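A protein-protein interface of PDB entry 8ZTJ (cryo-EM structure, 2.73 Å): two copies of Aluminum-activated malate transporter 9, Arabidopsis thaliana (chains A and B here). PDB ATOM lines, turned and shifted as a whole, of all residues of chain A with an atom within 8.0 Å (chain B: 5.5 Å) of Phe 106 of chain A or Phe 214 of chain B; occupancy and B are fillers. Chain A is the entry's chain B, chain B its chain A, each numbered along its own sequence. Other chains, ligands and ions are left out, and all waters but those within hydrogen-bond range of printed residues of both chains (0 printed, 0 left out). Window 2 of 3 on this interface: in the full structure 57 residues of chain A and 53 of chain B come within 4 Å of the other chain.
Printed residues of chain B within 4 Å of Thr 99 of chain A: Thr 173.
Ile 105 of chain A touches none of the printed residues of chain B.
Of the printed residues of chain B, Phe 106 of chain A touches Thr 173 and Phe 214.
Of the printed residues of chain B, Tyr 107 of chain A touches Glu 169 (3.4 Å).
Of the printed residues of chain B, Ile 122 of chain A touches Ile 211 (3.6 Å).
Of the printed residues of chain A, Glu 169 of chain B touches Tyr 107 (3.4 Å).
No residue of chain A comes within 4 Å of Gly 213 of chain B.
Phe 214 of chain B touches just one residue of chain A: Phe 106.
The nearest residue of chain B that does not touch Phe 106 of chain A is Glu 169 of chain B (4.1 Å).
Printed residues of chain B that touch a printed residue of chain A: Glu 169, Thr 173, Ile 211 and Phe 214.
Hydrophobic or aromatic side chains of chain B within 4 Å of the printed part of chain A: Ile 211 and Phe 214.
Among the printed residues, 5 pairs touch across the chains.
Among the printed residues, no Asp or Glu carboxylate lies within 4 Å of a Lys or Arg side-chain nitrogen of the other chain.
The backbone carbonyl oxygen (O) of Ile 211 of chain B sits at hydrogen-bond distance from the guanidinium group (NH1) of Arg 215 of chain B.
Among the printed residues, merely in contact across the chains: Tyr 107 of chain A with Glu 169 of chain B, Ile 122 of chain A with Ile 211 of chain B, Phe 106 of chain A with Phe 214 of chain B, Phe 106 of chain A with Thr 173 of chain B and Thr 99 of chain A with Thr 173 of chain B.
No position is printed for both chains.
Of the 5 pairs that touch across the chains among the printed residues, none has its exchanged pair printed and touching as well.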
ATOM      1  N   THR A  99      -3.536   0.500 -16.349  1.00  0.00           N
ATOM      2  CA  THR A  99      -2.321  -0.049 -16.939  1.00  0.00           C
ATOM      3  C   THR A  99      -1.113   0.830 -16.644  1.00  0.00           C
ATOM      4  O   THR A  99      -0.020   0.324 -16.368  1.00  0.00           O
ATOM      5  CB  THR A  99      -2.500  -0.217 -18.448  1.00  0.00           C
ATOM      6  OG1 THR A  99      -3.349  -1.341 -18.708  1.00  0.00           O
ATOM      7  CG2 THR A  99      -1.155  -0.437 -19.122  1.00  0.00           C
ATOM      8  N   ILE A 100      -1.286   2.153 -16.710  1.00  0.00           N
ATOM      9  CA  ILE A 100      -0.187   3.060 -16.387  1.00  0.00           C
ATOM     10  C   ILE A 100       0.269   2.847 -14.949  1.00  0.00           C
ATOM     11  O   ILE A 100       1.471   2.715 -14.664  1.00  0.00           O
ATOM     12  CB  ILE A 100      -0.602   4.521 -16.637  1.00  0.00           C
ATOM     13  CG1 ILE A 100      -0.740   4.790 -18.137  1.00  0.00           C
ATOM     14  CG2 ILE A 100       0.402   5.478 -16.012  1.00  0.00           C
ATOM     15  CD1 ILE A 100      -1.431   6.095 -18.459  1.00  0.00           C
ATOM     16  N   VAL A 101      -0.685   2.818 -14.015  1.00  0.00           N
ATOM     17  CA  VAL A 101      -0.314   2.644 -12.612  1.00  0.00           C
ATOM     18  C   VAL A 101       0.364   1.295 -12.402  1.00  0.00           C
ATOM     19  O   VAL A 101       1.343   1.183 -11.652  1.00  0.00           O
ATOM     20  CB  VAL A 101      -1.547   2.812 -11.704  1.00  0.00           C
ATOM     21  CG1 VAL A 101      -1.219   2.383 -10.285  1.00  0.00           C
ATOM     22  CG2 VAL A 101      -2.027   4.249 -11.729  1.00  0.00           C
ATOM     23  N   ALA A 102      -0.143   0.247 -13.055  1.00  0.00           N
ATOM     24  CA  ALA A 102       0.458  -1.076 -12.922  1.00  0.00           C
ATOM     25  C   ALA A 102       1.885  -1.095 -13.453  1.00  0.00           C
ATOM     26  O   ALA A 102       2.766  -1.727 -12.861  1.00  0.00           O
ATOM     27  CB  ALA A 102      -0.396  -2.118 -13.643  1.00  0.00           C
ATOM     28  N   LEU A 103       2.131  -0.427 -14.581  1.00  0.00           N
ATOM     29  CA  LEU A 103       3.487  -0.355 -15.113  1.00  0.00           C
ATOM     30  C   LEU A 103       4.423   0.346 -14.138  1.00  0.00           C
ATOM     31  O   LEU A 103       5.546  -0.116 -13.895  1.00  0.00           O
ATOM     32  CB  LEU A 103       3.487   0.364 -16.462  1.00  0.00           C
ATOM     33  CG  LEU A 103       3.146  -0.458 -17.704  1.00  0.00           C
ATOM     34  CD1 LEU A 103       3.186   0.417 -18.946  1.00  0.00           C
ATOM     35  CD2 LEU A 103       4.093  -1.636 -17.849  1.00  0.00           C
ATOM     36  N   LEU A 104       3.976   1.470 -13.569  1.00  0.00           N
ATOM     37  CA  LEU A 104       4.800   2.169 -12.586  1.00  0.00           C
ATOM     38  C   LEU A 104       5.067   1.309 -11.353  1.00  0.00           C
ATOM     39  O   LEU A 104       6.155   1.375 -10.768  1.00  0.00           O
ATOM     40  CB  LEU A 104       4.141   3.488 -12.184  1.00  0.00           C
ATOM     41  CG  LEU A 104       4.135   4.605 -13.228  1.00  0.00           C
ATOM     42  CD1 LEU A 104       2.996   5.576 -12.970  1.00  0.00           C
ATOM     43  CD2 LEU A 104       5.469   5.332 -13.232  1.00  0.00           C
ATOM     44  N   ILE A 105       4.091   0.495 -10.941  1.00  0.00           N
ATOM     45  CA  ILE A 105       4.311  -0.384  -9.792  1.00  0.00           C
ATOM     46  C   ILE A 105       5.216  -1.562 -10.136  1.00  0.00           C
ATOM     47  O   ILE A 105       5.930  -2.076  -9.266  1.00  0.00           O
ATOM     48  CB  ILE A 105       2.968  -0.870  -9.216  1.00  0.00           C
ATOM     49  CG1 ILE A 105       2.065   0.314  -8.875  1.00  0.00           C
ATOM     50  CG2 ILE A 105       3.198  -1.742  -7.993  1.00  0.00           C
ATOM     51  CD1 ILE A 105       0.668  -0.090  -8.458  1.00  0.00           C
ATOM     52  N   PHE A 106       5.209  -2.017 -11.388  1.00  0.00           N
ATOM     53  CA  PHE A 106       6.011  -3.174 -11.768  1.00  0.00           C
ATOM     54  C   PHE A 106       7.431  -2.818 -12.182  1.00  0.00           C
ATOM     55  O   PHE A 106       8.292  -3.704 -12.201  1.00  0.00           O
ATOM     56  CB  PHE A 106       5.331  -3.940 -12.908  1.00  0.00           C
ATOM     57  CG  PHE A 106       4.245  -4.871 -12.450  1.00  0.00           C
ATOM     58  CD1 PHE A 106       4.321  -5.487 -11.214  1.00  0.00           C
ATOM     59  CD2 PHE A 106       3.149  -5.129 -13.255  1.00  0.00           C
ATOM     60  CE1 PHE A 106       3.325  -6.344 -10.787  1.00  0.00           C
ATOM     61  CE2 PHE A 106       2.149  -5.985 -12.834  1.00  0.00           C
ATOM     62  CZ  PHE A 106       2.237  -6.593 -11.599  1.00  0.00           C
ATOM     63  N   TYR A 107       7.702  -1.556 -12.509  1.00  0.00           N
ATOM     64  CA  TYR A 107       9.045  -1.174 -12.926  1.00  0.00           C
ATOM     65  C   TYR A 107       9.588  -0.056 -12.045  1.00  0.00           C
ATOM     66  O   TYR A 107      10.116   0.942 -12.545  1.00  0.00           O
ATOM     67  CB  TYR A 107       9.053  -0.763 -14.400  1.00  0.00           C
ATOM     68  CG  TYR A 107       8.852  -1.923 -15.349  1.00  0.00           C
ATOM     69  CD1 TYR A 107       9.683  -3.035 -15.300  1.00  0.00           C
ATOM     70  CD2 TYR A 107       7.831  -1.911 -16.289  1.00  0.00           C
ATOM     71  CE1 TYR A 107       9.507  -4.100 -16.161  1.00  0.00           C
ATOM     72  CE2 TYR A 107       7.647  -2.974 -17.155  1.00  0.00           C
ATOM     73  CZ  TYR A 107       8.487  -4.065 -17.086  1.00  0.00           C
ATOM     74  OH  TYR A 107       8.307  -5.123 -17.946  1.00  0.00           O
ATOM     75  N   GLN A 108       9.459  -0.222 -10.733  1.00  0.00           N
ATOM     76  CA  GLN A 108       9.833   0.791  -9.759  1.00  0.00           C
ATOM     77  C   GLN A 108      11.216   0.504  -9.187  1.00  0.00           C
ATOM     78  O   GLN A 108      11.641  -0.649  -9.083  1.00  0.00           O
ATOM     79  CB  GLN A 108       8.811   0.858  -8.621  1.00  0.00           C
ATOM     80  CG  GLN A 108       8.867  -0.328  -7.673  1.00  0.00           C
ATOM     81  CD  GLN A 108       7.703  -0.354  -6.699  1.00  0.00           C
ATOM     82  OE1 GLN A 108       7.150   0.687  -6.348  1.00  0.00           O
ATOM     83  NE2 GLN A 108       7.329  -1.548  -6.256  1.00  0.00           N
ATOM     84  N   GLU A 109      11.913   1.570  -8.819  1.00  0.00           N
ATOM     85  CA  GLU A 109      13.245   1.447  -8.236  1.00  0.00           C
ATOM     86  C   GLU A 109      13.146   0.804  -6.859  1.00  0.00           C
ATOM     87  O   GLU A 109      12.407   1.308  -6.003  1.00  0.00           O
ATOM     88  CB  GLU A 109      13.907   2.819  -8.141  1.00  0.00           C
ATOM     89  CG  GLU A 109      15.426   2.794  -8.229  1.00  0.00           C
ATOM     90  CD  GLU A 109      16.067   1.987  -7.117  1.00  0.00           C
ATOM     91  OE1 GLU A 109      15.736   2.232  -5.938  1.00  0.00           O
ATOM     92  OE2 GLU A 109      16.903   1.111  -7.423  1.00  0.00           O
ATOM     93  N   SER A 118       2.635  -0.005  -2.523  1.00  0.00           N
ATOM     94  CA  SER A 118       2.367   0.510  -3.862  1.00  0.00           C
ATOM     95  C   SER A 118       0.926   0.259  -4.279  1.00  0.00           C
ATOM     96  O   SER A 118       0.388   0.983  -5.123  1.00  0.00           O
ATOM     97  CB  SER A 118       3.324  -0.124  -4.870  1.00  0.00           C
ATOM     98  OG  SER A 118       4.607   0.471  -4.803  1.00  0.00           O
ATOM     99  N   ILE A 122      -3.331   1.984  -6.999  1.00  0.00           N
ATOM    100  CA  ILE A 122      -4.199   1.427  -8.028  1.00  0.00           C
ATOM    101  C   ILE A 122      -5.653   1.289  -7.586  1.00  0.00           C
ATOM    102  O   ILE A 122      -6.533   1.112  -8.440  1.00  0.00           O
ATOM    103  CB  ILE A 122      -3.671   0.058  -8.493  1.00  0.00           C
ATOM    104  CG1 ILE A 122      -4.317  -0.345  -9.819  1.00  0.00           C
ATOM    105  CG2 ILE A 122      -3.920  -1.000  -7.432  1.00  0.00           C
ATOM    106  CD1 ILE A 122      -3.367  -1.021 -10.778  1.00  0.00           C
ATOM    107  N   GLU B 168       6.124 -12.046 -18.069  1.00  0.00           N
ATOM    108  CA  GLU B 168       5.130 -12.307 -17.035  1.00  0.00           C
ATOM    109  C   GLU B 168       4.368 -11.045 -16.638  1.00  0.00           C
ATOM    110  O   GLU B 168       3.131 -11.037 -16.623  1.00  0.00           O
ATOM    111  CB  GLU B 168       5.810 -12.924 -15.809  1.00  0.00           C
ATOM    112  CG  GLU B 168       5.050 -14.083 -15.191  1.00  0.00           C
ATOM    113  CD  GLU B 168       5.330 -14.235 -13.708  1.00  0.00           C
ATOM    114  OE1 GLU B 168       6.517 -14.214 -13.322  1.00  0.00           O
ATOM    115  OE2 GLU B 168       4.362 -14.374 -12.930  1.00  0.00           O
ATOM    116  N   GLU B 169       5.093  -9.970 -16.318  1.00  0.00           N
ATOM    117  CA  GLU B 169       4.439  -8.715 -15.964  1.00  0.00           C
ATOM    118  C   GLU B 169       3.685  -8.113 -17.142  1.00  0.00           C
ATOM    119  O   GLU B 169       2.643  -7.476 -16.947  1.00  0.00           O
ATOM    120  CB  GLU B 169       5.470  -7.728 -15.422  1.00  0.00           C
ATOM    121  CG  GLU B 169       6.756  -7.673 -16.225  1.00  0.00           C
ATOM    122  CD  GLU B 169       7.800  -8.645 -15.713  1.00  0.00           C
ATOM    123  OE1 GLU B 169       7.413  -9.683 -15.138  1.00  0.00           O
ATOM    124  OE2 GLU B 169       9.008  -8.373 -15.885  1.00  0.00           O
ATOM    125  N   CYS B 172       0.463  -9.888 -17.079  1.00  0.00           N
ATOM    126  CA  CYS B 172      -0.375  -9.413 -15.982  1.00  0.00           C
ATOM    127  C   CYS B 172      -1.023  -8.070 -16.307  1.00  0.00           C
ATOM    128  O   CYS B 172      -2.219  -7.879 -16.058  1.00  0.00           O
ATOM    129  CB  CYS B 172       0.455  -9.312 -14.703  1.00  0.00           C
ATOM    130  SG  CYS B 172       0.709 -10.886 -13.848  1.00  0.00           S
ATOM    131  N   THR B 173      -0.254  -7.124 -16.853  1.00  0.00           N
ATOM    132  CA  THR B 173      -0.824  -5.815 -17.173  1.00  0.00           C
ATOM    133  C   THR B 173      -1.809  -5.886 -18.337  1.00  0.00           C
ATOM    134  O   THR B 173      -2.811  -5.153 -18.349  1.00  0.00           O
ATOM    135  CB  THR B 173       0.281  -4.807 -17.488  1.00  0.00           C
ATOM    136  OG1 THR B 173       0.745  -5.001 -18.829  1.00  0.00           O
ATOM    137  CG2 THR B 173       1.445  -4.961 -16.523  1.00  0.00           C
ATOM    138  N   ILE B 209      -5.256  -8.809  -5.437  1.00  0.00           N
ATOM    139  CA  ILE B 209      -4.666 -10.142  -5.390  1.00  0.00           C
ATOM    140  C   ILE B 209      -3.610 -10.303  -6.475  1.00  0.00           C
ATOM    141  O   ILE B 209      -2.570 -10.936  -6.254  1.00  0.00           O
ATOM    142  CB  ILE B 209      -5.757 -11.221  -5.498  1.00  0.00           C
ATOM    143  CG1 ILE B 209      -6.557 -11.304  -4.198  1.00  0.00           C
ATOM    144  CG2 ILE B 209      -5.140 -12.570  -5.828  1.00  0.00           C
ATOM    145  CD1 ILE B 209      -7.652 -12.339  -4.232  1.00  0.00           C
ATOM    146  N   LEU B 210      -3.849  -9.744  -7.665  1.00  0.00           N
ATOM    147  CA  LEU B 210      -2.852  -9.857  -8.725  1.00  0.00           C
ATOM    148  C   LEU B 210      -1.567  -9.121  -8.369  1.00  0.00           C
ATOM    149  O   LEU B 210      -0.469  -9.648  -8.582  1.00  0.00           O
ATOM    150  CB  LEU B 210      -3.420  -9.338 -10.045  1.00  0.00           C
ATOM    151  CG  LEU B 210      -2.949 -10.094 -11.288  1.00  0.00           C
ATOM    152  CD1 LEU B 210      -3.406 -11.541 -11.245  1.00  0.00           C
ATOM    153  CD2 LEU B 210      -3.441  -9.410 -12.553  1.00  0.00           C
ATOM    154  N   ILE B 211      -1.674  -7.905  -7.828  1.00  0.00           N
ATOM    155  CA  ILE B 211      -0.469  -7.115  -7.594  1.00  0.00           C
ATOM    156  C   ILE B 211       0.265  -7.541  -6.326  1.00  0.00           C
ATOM    157  O   ILE B 211       1.492  -7.414  -6.251  1.00  0.00           O
ATOM    158  CB  ILE B 211      -0.813  -5.616  -7.556  1.00  0.00           C
ATOM    159  CG1 ILE B 211      -1.281  -5.144  -8.935  1.00  0.00           C
ATOM    160  CG2 ILE B 211       0.379  -4.806  -7.075  1.00  0.00           C
ATOM    161  CD1 ILE B 211      -1.883  -3.760  -8.933  1.00  0.00           C
ATOM    162  N   SER B 212      -0.444  -8.052  -5.321  1.00  0.00           N
ATOM    163  CA  SER B 212       0.198  -8.378  -4.055  1.00  0.00           C
ATOM    164  C   SER B 212       0.918  -9.719  -4.066  1.00  0.00           C
ATOM    165  O   SER B 212       1.716  -9.979  -3.159  1.00  0.00           O
ATOM    166  CB  SER B 212      -0.837  -8.369  -2.928  1.00  0.00           C
ATOM    167  OG  SER B 212      -1.493  -7.117  -2.857  1.00  0.00           O
ATOM    168  N   GLY B 213       0.668 -10.570  -5.054  1.00  0.00           N
ATOM    169  CA  GLY B 213       1.307 -11.870  -5.087  1.00  0.00           C
ATOM    170  C   GLY B 213       2.415 -11.989  -6.110  1.00  0.00           C
ATOM    171  O   GLY B 213       3.062 -13.034  -6.211  1.00  0.00           O
ATOM    172  N   PHE B 214       2.654 -10.922  -6.873  1.00  0.00           N
ATOM    173  CA  PHE B 214       3.648 -10.993  -7.938  1.00  0.00           C
ATOM    174  C   PHE B 214       5.028 -11.330  -7.386  1.00  0.00           C
ATOM    175  O   PHE B 214       5.735 -12.182  -7.938  1.00  0.00           O
ATOM    176  CB  PHE B 214       3.686  -9.676  -8.710  1.00  0.00           C
ATOM    177  CG  PHE B 214       4.632  -9.685  -9.875  1.00  0.00           C
ATOM    178  CD1 PHE B 214       4.365 -10.455 -10.994  1.00  0.00           C
ATOM    179  CD2 PHE B 214       5.788  -8.926  -9.852  1.00  0.00           C
ATOM    180  CE1 PHE B 214       5.231 -10.467 -12.067  1.00  0.00           C
ATOM    181  CE2 PHE B 214       6.659  -8.933 -10.923  1.00  0.00           C
ATOM    182  CZ  PHE B 214       6.380  -9.706 -12.032  1.00  0.00           C
ATOM    183  N   ARG B 215       5.425 -10.679  -6.297  1.00  0.00           N
ATOM    184  CA  ARG B 215       6.730 -10.926  -5.701  1.00  0.00           C
ATOM    185  C   ARG B 215       6.675 -12.151  -4.796  1.00  0.00           C
ATOM    186  O   ARG B 215       5.787 -12.269  -3.947  1.00  0.00           O
ATOM    187  CB  ARG B 215       7.191  -9.703  -4.910  1.00  0.00           C
ATOM    188  CG  ARG B 215       6.139  -9.142  -3.965  1.00  0.00           C
ATOM    189  CD  ARG B 215       5.270  -8.106  -4.660  1.00  0.00           C
ATOM    190  NE  ARG B 215       4.609  -7.216  -3.712  1.00  0.00           N
ATOM    191  CZ  ARG B 215       4.126  -6.021  -4.020  1.00  0.00           C
ATOM    192  NH1 ARG B 215       4.210  -5.537  -5.249  1.00  0.00           N
ATOM    193  NH2 ARG B 215       3.543  -5.291  -3.072  1.00  0.00           N
ATOM    194  N   THR B 216       7.629 -13.065  -4.983  1.00  0.00           N
ATOM    195  CA  THR B 216       7.810 -14.209  -4.095  1.00  0.00           C
ATOM    196  C   THR B 216       6.622 -15.165  -4.134  1.00  0.00           C
ATOM    197  O   THR B 216       6.329 -15.835  -3.142  1.00  0.00           O
ATOM    198  CB  THR B 216       8.072 -13.758  -2.655  1.00  0.00           C
ATOM    199  OG1 THR B 216       6.830 -13.419  -2.025  1.00  0.00           O
ATOM    200  CG2 THR B 216       8.996 -12.547  -2.634  1.00  0.00           C
ATOM    201  N   GLY B 217       5.945 -15.259  -5.273  1.00  0.00           N
ATOM    202  CA  GLY B 217       4.745 -16.077  -5.338  1.00  0.00           C
ATOM    203  C   GLY B 217       3.752 -15.672  -4.267  1.00  0.00           C
ATOM    204  O   GLY B 217       3.379 -14.500  -4.146  1.00  0.00           O
ATOM    205  N   PHE B 219       0.390 -16.596  -3.679  1.00  0.00           N
ATOM    206  CA  PHE B 219      -0.932 -16.220  -4.160  1.00  0.00           C
ATOM    207  C   PHE B 219      -2.068 -16.845  -3.363  1.00  0.00           C
ATOM    208  O   PHE B 219      -3.120 -16.216  -3.214  1.00  0.00           O
ATOM    209  CB  PHE B 219      -1.096 -16.607  -5.635  1.00  0.00           C
ATOM    210  CG  PHE B 219      -0.552 -15.591  -6.597  1.00  0.00           C
ATOM    211  CD1 PHE B 219       0.795 -15.575  -6.920  1.00  0.00           C
ATOM    212  CD2 PHE B 219      -1.384 -14.647  -7.172  1.00  0.00           C
ATOM    213  CE1 PHE B 219       1.297 -14.642  -7.806  1.00  0.00           C
ATOM    214  CE2 PHE B 219      -0.885 -13.708  -8.055  1.00  0.00           C
ATOM    215  CZ  PHE B 219       0.458 -13.707  -8.373  1.00  0.00           C
